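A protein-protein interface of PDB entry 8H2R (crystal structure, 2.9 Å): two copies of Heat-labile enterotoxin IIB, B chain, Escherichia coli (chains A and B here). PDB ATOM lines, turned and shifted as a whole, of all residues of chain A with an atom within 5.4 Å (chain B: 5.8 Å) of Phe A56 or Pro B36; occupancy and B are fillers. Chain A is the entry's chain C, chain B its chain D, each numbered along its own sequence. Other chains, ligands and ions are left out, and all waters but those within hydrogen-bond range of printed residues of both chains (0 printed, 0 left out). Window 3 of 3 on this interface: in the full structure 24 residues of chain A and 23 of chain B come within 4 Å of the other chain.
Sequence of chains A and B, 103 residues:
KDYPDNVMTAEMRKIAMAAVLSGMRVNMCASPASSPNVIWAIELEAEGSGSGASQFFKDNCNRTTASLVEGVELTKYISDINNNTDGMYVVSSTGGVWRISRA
The side-chain amide oxygen (OD1) of Asn A60 sits close to the backbone carbonyl oxygen (O) of Phe A56, at 2.5 Å. The side-chain hydroxyl of Tyr B89 sits at hydrogen-bond distance from the guanidinium group of Arg B99. N of Phe A57 sits at hydrogen-bond distance from OG of Ser A54 (3.1 Å). The backbone carbonyl oxygen (O) of Tyr B89 is in hydrogen-bond range of the backbone NH (N) of Ile B78 (2.7 Å).
Among the printed residues, pairs that only touch across the chains: Ser A54 with Ile B78, Phe A56 with Pro B36, Phe A56 with Tyr B89, Phe A56 with Val B97, Phe A57 with Ile B78 and Asn A60 with Thr B85.
Of the printed residues of chain B, Ser A54 touches Ile B78 (3.9 Å). Gln A55 touches none of the printed residues of chain B. Phe A56 touches just these residues of chain B: Pro B36 (3.8 Å), Tyr B89 (3.6 Å) and Val B97 (3.5 Å). Pro B36 touches one residue of chain A. Printed residues of chain A within 4 Å of Ile B78: Ser A54 and Phe A57. Of the printed residues of chain A, Thr B85 touches Asn A60 (3.0 Å). Printed residues of chain A within 4 Å of Tyr B89: Phe A56 (3.6 Å). The nearest residue of chain B that does not touch Phe A56 is Ile B78 (4.1 Å). The nearest printed residue of chain A that does not touch Pro B36 is Asn A60 (7.2 Å).
Hydrophobic or aromatic side chains of chain B within 4 Å of the printed part of chain A: Pro B36, Ile B78, Tyr B89 and Val B97. Of the 7 printed residues of chain A, 4 touch a printed residue of chain B. Printed residues of chain A that touch a printed residue of chain B: Ser A54, Phe A56, Phe A57 and Asn A60. Hydrophobic or aromatic side chains of chain A that line the printed part of chain B: Phe A56 and Phe A57. Among the printed residues, 6 pairs touch across the chains. Among the printed residues, no Asp or Glu carboxylate lies within 4 Å of a Lys or Arg side-chain nitrogen of the other chain.
No position is printed for both chains.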
ATOM      1  N   SER A  54       1.398   8.065 -15.098  1.00  0.00           N
ATOM      2  CA  SER A  54       1.830   6.781 -14.571  1.00  0.00           C
ATOM      3  C   SER A  54       0.766   5.742 -14.863  1.00  0.00           C
ATOM      4  O   SER A  54      -0.421   6.062 -14.975  1.00  0.00           O
ATOM      5  CB  SER A  54       2.093   6.857 -13.063  1.00  0.00           C
ATOM      6  OG  SER A  54       0.914   7.194 -12.353  1.00  0.00           O
ATOM      7  N   GLN A  55       1.208   4.488 -15.006  1.00  0.00           N
ATOM      8  CA  GLN A  55       0.266   3.420 -15.288  1.00  0.00           C
ATOM      9  C   GLN A  55      -0.810   3.371 -14.226  1.00  0.00           C
ATOM     10  O   GLN A  55      -2.000   3.355 -14.542  1.00  0.00           O
ATOM     11  CB  GLN A  55       0.976   2.075 -15.394  1.00  0.00           C
ATOM     12  CG  GLN A  55       0.183   1.066 -16.236  1.00  0.00           C
ATOM     13  CD  GLN A  55      -0.714   1.756 -17.267  1.00  0.00           C
ATOM     14  OE1 GLN A  55      -0.236   2.448 -18.171  1.00  0.00           O
ATOM     15  NE2 GLN A  55      -2.018   1.540 -17.152  1.00  0.00           N
ATOM     16  N   PHE A  56      -0.413   3.384 -12.958  1.00  0.00           N
ATOM     17  CA  PHE A  56      -1.410   3.508 -11.909  1.00  0.00           C
ATOM     18  C   PHE A  56      -2.381   4.632 -12.237  1.00  0.00           C
ATOM     19  O   PHE A  56      -3.571   4.387 -12.428  1.00  0.00           O
ATOM     20  CB  PHE A  56      -0.751   3.731 -10.551  1.00  0.00           C
ATOM     21  CG  PHE A  56      -1.734   3.789  -9.421  1.00  0.00           C
ATOM     22  CD1 PHE A  56      -2.160   5.007  -8.910  1.00  0.00           C
ATOM     23  CD2 PHE A  56      -2.265   2.628  -8.894  1.00  0.00           C
ATOM     24  CE1 PHE A  56      -3.073   5.060  -7.874  1.00  0.00           C
ATOM     25  CE2 PHE A  56      -3.184   2.674  -7.867  1.00  0.00           C
ATOM     26  CZ  PHE A  56      -3.588   3.892  -7.355  1.00  0.00           C
ATOM     27  N   PHE A  57      -1.877   5.859 -12.402  1.00  0.00           N
ATOM     28  CA  PHE A  57      -2.784   6.979 -12.642  1.00  0.00           C
ATOM     29  C   PHE A  57      -3.737   6.696 -13.788  1.00  0.00           C
ATOM     30  O   PHE A  57      -4.918   7.047 -13.714  1.00  0.00           O
ATOM     31  CB  PHE A  57      -2.027   8.275 -12.927  1.00  0.00           C
ATOM     32  CG  PHE A  57      -2.902   9.510 -12.820  1.00  0.00           C
ATOM     33  CD1 PHE A  57      -3.856   9.810 -13.787  1.00  0.00           C
ATOM     34  CD2 PHE A  57      -2.804  10.350 -11.723  1.00  0.00           C
ATOM     35  CE1 PHE A  57      -4.673  10.938 -13.663  1.00  0.00           C
ATOM     36  CE2 PHE A  57      -3.619  11.484 -11.602  1.00  0.00           C
ATOM     37  CZ  PHE A  57      -4.546  11.772 -12.573  1.00  0.00           C
ATOM     38  N   LYS A  58      -3.254   6.044 -14.849  1.00  0.00           N
ATOM     39  CA  LYS A  58      -4.091   5.840 -16.031  1.00  0.00           C
ATOM     40  C   LYS A  58      -5.318   5.002 -15.718  1.00  0.00           C
ATOM     41  O   LYS A  58      -6.428   5.334 -16.144  1.00  0.00           O
ATOM     42  CB  LYS A  58      -3.286   5.184 -17.144  1.00  0.00           C
ATOM     43  CG  LYS A  58      -2.607   6.195 -18.040  1.00  0.00           C
ATOM     44  CD  LYS A  58      -1.651   5.548 -19.007  1.00  0.00           C
ATOM     45  CE  LYS A  58      -2.232   5.596 -20.392  1.00  0.00           C
ATOM     46  NZ  LYS A  58      -1.221   5.140 -21.361  1.00  0.00           N
ATOM     47  N   ASP A  59      -5.141   3.927 -14.954  1.00  0.00           N
ATOM     48  CA  ASP A  59      -6.206   2.945 -14.783  1.00  0.00           C
ATOM     49  C   ASP A  59      -7.312   3.445 -13.863  1.00  0.00           C
ATOM     50  O   ASP A  59      -8.476   3.053 -14.028  1.00  0.00           O
ATOM     51  CB  ASP A  59      -5.597   1.649 -14.276  1.00  0.00           C
ATOM     52  CG  ASP A  59      -4.332   1.291 -15.027  1.00  0.00           C
ATOM     53  OD1 ASP A  59      -4.248   1.640 -16.223  1.00  0.00           O
ATOM     54  OD2 ASP A  59      -3.414   0.696 -14.423  1.00  0.00           O
ATOM     55  N   ASN A  60      -6.987   4.320 -12.909  1.00  0.00           N
ATOM     56  CA  ASN A  60      -8.066   4.889 -12.122  1.00  0.00           C
ATOM     57  C   ASN A  60      -8.858   5.917 -12.913  1.00  0.00           C
ATOM     58  O   ASN A  60      -9.930   6.332 -12.461  1.00  0.00           O
ATOM     59  CB  ASN A  60      -7.552   5.512 -10.818  1.00  0.00           C
ATOM     60  CG  ASN A  60      -6.314   4.803 -10.261  1.00  0.00           C
ATOM     61  OD1 ASN A  60      -5.189   5.107 -10.644  1.00  0.00           O
ATOM     62  ND2 ASN A  60      -6.528   3.808  -9.412  1.00  0.00           N
ATOM     63  N   SER B  31       3.434  -2.227   3.955  1.00  0.00           N
ATOM     64  CA  SER B  31       2.745  -3.485   4.178  1.00  0.00           C
ATOM     65  C   SER B  31       2.234  -4.015   2.845  1.00  0.00           C
ATOM     66  O   SER B  31       1.288  -3.428   2.293  1.00  0.00           O
ATOM     67  CB  SER B  31       1.594  -3.279   5.141  1.00  0.00           C
ATOM     68  OG  SER B  31       0.563  -4.195   4.876  1.00  0.00           O
ATOM     69  N   SER B  34      -1.635  -4.958   1.194  1.00  0.00           N
ATOM     70  CA  SER B  34      -2.484  -4.189   0.295  1.00  0.00           C
ATOM     71  C   SER B  34      -1.742  -3.948  -1.022  1.00  0.00           C
ATOM     72  O   SER B  34      -0.579  -4.324  -1.195  1.00  0.00           O
ATOM     73  CB  SER B  34      -2.917  -2.856   0.941  1.00  0.00           C
ATOM     74  OG  SER B  34      -3.131  -2.988   2.335  1.00  0.00           O
ATOM     75  N   SER B  35      -2.434  -3.307  -1.968  1.00  0.00           N
ATOM     76  CA  SER B  35      -1.832  -2.981  -3.251  1.00  0.00           C
ATOM     77  C   SER B  35      -2.534  -1.760  -3.841  1.00  0.00           C
ATOM     78  O   SER B  35      -3.688  -1.863  -4.273  1.00  0.00           O
ATOM     79  CB  SER B  35      -1.905  -4.183  -4.194  1.00  0.00           C
ATOM     80  OG  SER B  35      -0.770  -4.242  -5.048  1.00  0.00           O
ATOM     81  N   PRO B  36      -1.888  -0.578  -3.871  1.00  0.00           N
ATOM     82  CA  PRO B  36      -0.501  -0.284  -3.471  1.00  0.00           C
ATOM     83  C   PRO B  36      -0.188  -0.634  -2.005  1.00  0.00           C
ATOM     84  O   PRO B  36      -1.071  -0.550  -1.134  1.00  0.00           O
ATOM     85  CB  PRO B  36      -0.380   1.232  -3.726  1.00  0.00           C
ATOM     86  CG  PRO B  36      -1.500   1.591  -4.657  1.00  0.00           C
ATOM     87  CD  PRO B  36      -2.601   0.634  -4.318  1.00  0.00           C
ATOM     88  N   ASN B  37       1.047  -1.076  -1.733  1.00  0.00           N
ATOM     89  CA  ASN B  37       1.477  -1.317  -0.362  1.00  0.00           C
ATOM     90  C   ASN B  37       1.368  -0.024   0.424  1.00  0.00           C
ATOM     91  O   ASN B  37       1.973   0.986   0.053  1.00  0.00           O
ATOM     92  CB  ASN B  37       2.915  -1.848  -0.330  1.00  0.00           C
ATOM     93  CG  ASN B  37       3.111  -3.054  -1.228  1.00  0.00           C
ATOM     94  OD1 ASN B  37       2.142  -3.670  -1.667  1.00  0.00           O
ATOM     95  ND2 ASN B  37       4.364  -3.394  -1.514  1.00  0.00           N
ATOM     96  N   VAL B  38       0.579  -0.049   1.501  1.00  0.00           N
ATOM     97  CA  VAL B  38       0.297   1.163   2.256  1.00  0.00           C
ATOM     98  C   VAL B  38       1.539   1.601   3.019  1.00  0.00           C
ATOM     99  O   VAL B  38       2.259   0.780   3.603  1.00  0.00           O
ATOM    100  CB  VAL B  38      -0.908   0.935   3.183  1.00  0.00           C
ATOM    101  CG1 VAL B  38      -0.834   1.816   4.406  1.00  0.00           C
ATOM    102  CG2 VAL B  38      -2.208   1.211   2.417  1.00  0.00           C
ATOM    103  N   ILE B  78       0.497  11.895  -6.316  1.00  0.00           N
ATOM    104  CA  ILE B  78      -0.896  11.833  -6.773  1.00  0.00           C
ATOM    105  C   ILE B  78      -1.845  12.162  -5.624  1.00  0.00           C
ATOM    106  O   ILE B  78      -1.736  11.573  -4.540  1.00  0.00           O
ATOM    107  CB  ILE B  78      -1.261  10.449  -7.352  1.00  0.00           C
ATOM    108  CG1 ILE B  78      -0.550  10.170  -8.674  1.00  0.00           C
ATOM    109  CG2 ILE B  78      -2.759  10.340  -7.547  1.00  0.00           C
ATOM    110  CD1 ILE B  78      -0.313   8.692  -8.938  1.00  0.00           C
ATOM    111  N   THR B  85     -11.156   5.369  -5.877  1.00  0.00           N
ATOM    112  CA  THR B  85      -9.728   5.639  -5.775  1.00  0.00           C
ATOM    113  C   THR B  85      -9.497   6.938  -5.000  1.00  0.00           C
ATOM    114  O   THR B  85      -8.794   7.849  -5.437  1.00  0.00           O
ATOM    115  CB  THR B  85      -9.113   5.669  -7.165  1.00  0.00           C
ATOM    116  OG1 THR B  85     -10.014   6.326  -8.061  1.00  0.00           O
ATOM    117  CG2 THR B  85      -8.934   4.252  -7.646  1.00  0.00           C
ATOM    118  N   TYR B  89      -1.089   9.014  -3.243  1.00  0.00           N
ATOM    119  CA  TYR B  89      -0.214   8.019  -3.849  1.00  0.00           C
ATOM    120  C   TYR B  89       1.096   8.659  -4.275  1.00  0.00           C
ATOM    121  O   TYR B  89       1.146   9.847  -4.626  1.00  0.00           O
ATOM    122  CB  TYR B  89      -0.882   7.313  -5.063  1.00  0.00           C
ATOM    123  CG  TYR B  89      -2.197   6.646  -4.702  1.00  0.00           C
ATOM    124  CD1 TYR B  89      -2.223   5.352  -4.188  1.00  0.00           C
ATOM    125  CD2 TYR B  89      -3.409   7.329  -4.827  1.00  0.00           C
ATOM    126  CE1 TYR B  89      -3.421   4.751  -3.827  1.00  0.00           C
ATOM    127  CE2 TYR B  89      -4.610   6.735  -4.462  1.00  0.00           C
ATOM    128  CZ  TYR B  89      -4.605   5.447  -3.966  1.00  0.00           C
ATOM    129  OH  TYR B  89      -5.780   4.850  -3.601  1.00  0.00           O
ATOM    130  N   VAL B  91       4.739   7.525  -6.624  1.00  0.00           N
ATOM    131  CA  VAL B  91       5.247   6.622  -7.641  1.00  0.00           C
ATOM    132  C   VAL B  91       6.750   6.821  -7.764  1.00  0.00           C
ATOM    133  O   VAL B  91       7.262   7.939  -7.636  1.00  0.00           O
ATOM    134  CB  VAL B  91       4.552   6.858  -9.005  1.00  0.00           C
ATOM    135  CG1 VAL B  91       4.848   5.706  -9.950  1.00  0.00           C
ATOM    136  CG2 VAL B  91       3.029   7.089  -8.832  1.00  0.00           C
ATOM    137  N   VAL B  97       4.218   1.764  -7.025  1.00  0.00           N
ATOM    138  CA  VAL B  97       3.145   2.618  -6.541  1.00  0.00           C
ATOM    139  C   VAL B  97       2.872   2.249  -5.091  1.00  0.00           C
ATOM    140  O   VAL B  97       2.727   1.065  -4.764  1.00  0.00           O
ATOM    141  CB  VAL B  97       1.878   2.492  -7.416  1.00  0.00           C
ATOM    142  CG1 VAL B  97       1.309   1.080  -7.382  1.00  0.00           C
ATOM    143  CG2 VAL B  97       0.835   3.504  -7.017  1.00  0.00           C
ATOM    144  N   TRP B  98       2.858   3.255  -4.211  1.00  0.00           N
ATOM    145  CA  TRP B  98       2.526   3.049  -2.809  1.00  0.00           C
ATOM    146  C   TRP B  98       1.405   3.981  -2.415  1.00  0.00           C
ATOM    147  O   TRP B  98       1.283   5.078  -2.951  1.00  0.00           O
ATOM    148  CB  TRP B  98       3.687   3.300  -1.880  1.00  0.00           C
ATOM    149  CG  TRP B  98       4.857   2.416  -2.071  1.00  0.00           C
ATOM    150  CD1 TRP B  98       5.249   1.395  -1.259  1.00  0.00           C
ATOM    151  CD2 TRP B  98       5.824   2.499  -3.113  1.00  0.00           C
ATOM    152  NE1 TRP B  98       6.400   0.821  -1.744  1.00  0.00           N
ATOM    153  CE2 TRP B  98       6.773   1.483  -2.884  1.00  0.00           C
ATOM    154  CE3 TRP B  98       5.974   3.319  -4.225  1.00  0.00           C
ATOM    155  CZ2 TRP B  98       7.865   1.273  -3.729  1.00  0.00           C
ATOM    156  CZ3 TRP B  98       7.055   3.115  -5.058  1.00  0.00           C
ATOM    157  CH2 TRP B  98       7.992   2.104  -4.807  1.00  0.00           C
ATOM    158  N   ARG B  99       0.585   3.527  -1.481  1.00  0.00           N
ATOM    159  CA  ARG B  99      -0.458   4.353  -0.904  1.00  0.00           C
ATOM    160  C   ARG B  99       0.040   4.912   0.410  1.00  0.00           C
ATOM    161  O   ARG B  99       0.786   4.254   1.145  1.00  0.00           O
ATOM    162  CB  ARG B  99      -1.753   3.579  -0.666  1.00  0.00           C
ATOM    163  CG  ARG B  99      -2.946   4.464  -0.311  1.00  0.00           C
ATOM    164  CD  ARG B  99      -4.217   3.633  -0.211  1.00  0.00           C
ATOM    165  NE  ARG B  99      -4.561   2.992  -1.478  1.00  0.00           N
ATOM    166  CZ  ARG B  99      -5.008   1.747  -1.576  1.00  0.00           C
ATOM    167  NH1 ARG B  99      -5.168   0.981  -0.507  1.00  0.00           N
ATOM    168  NH2 ARG B  99      -5.292   1.251  -2.777  1.00  0.00           N
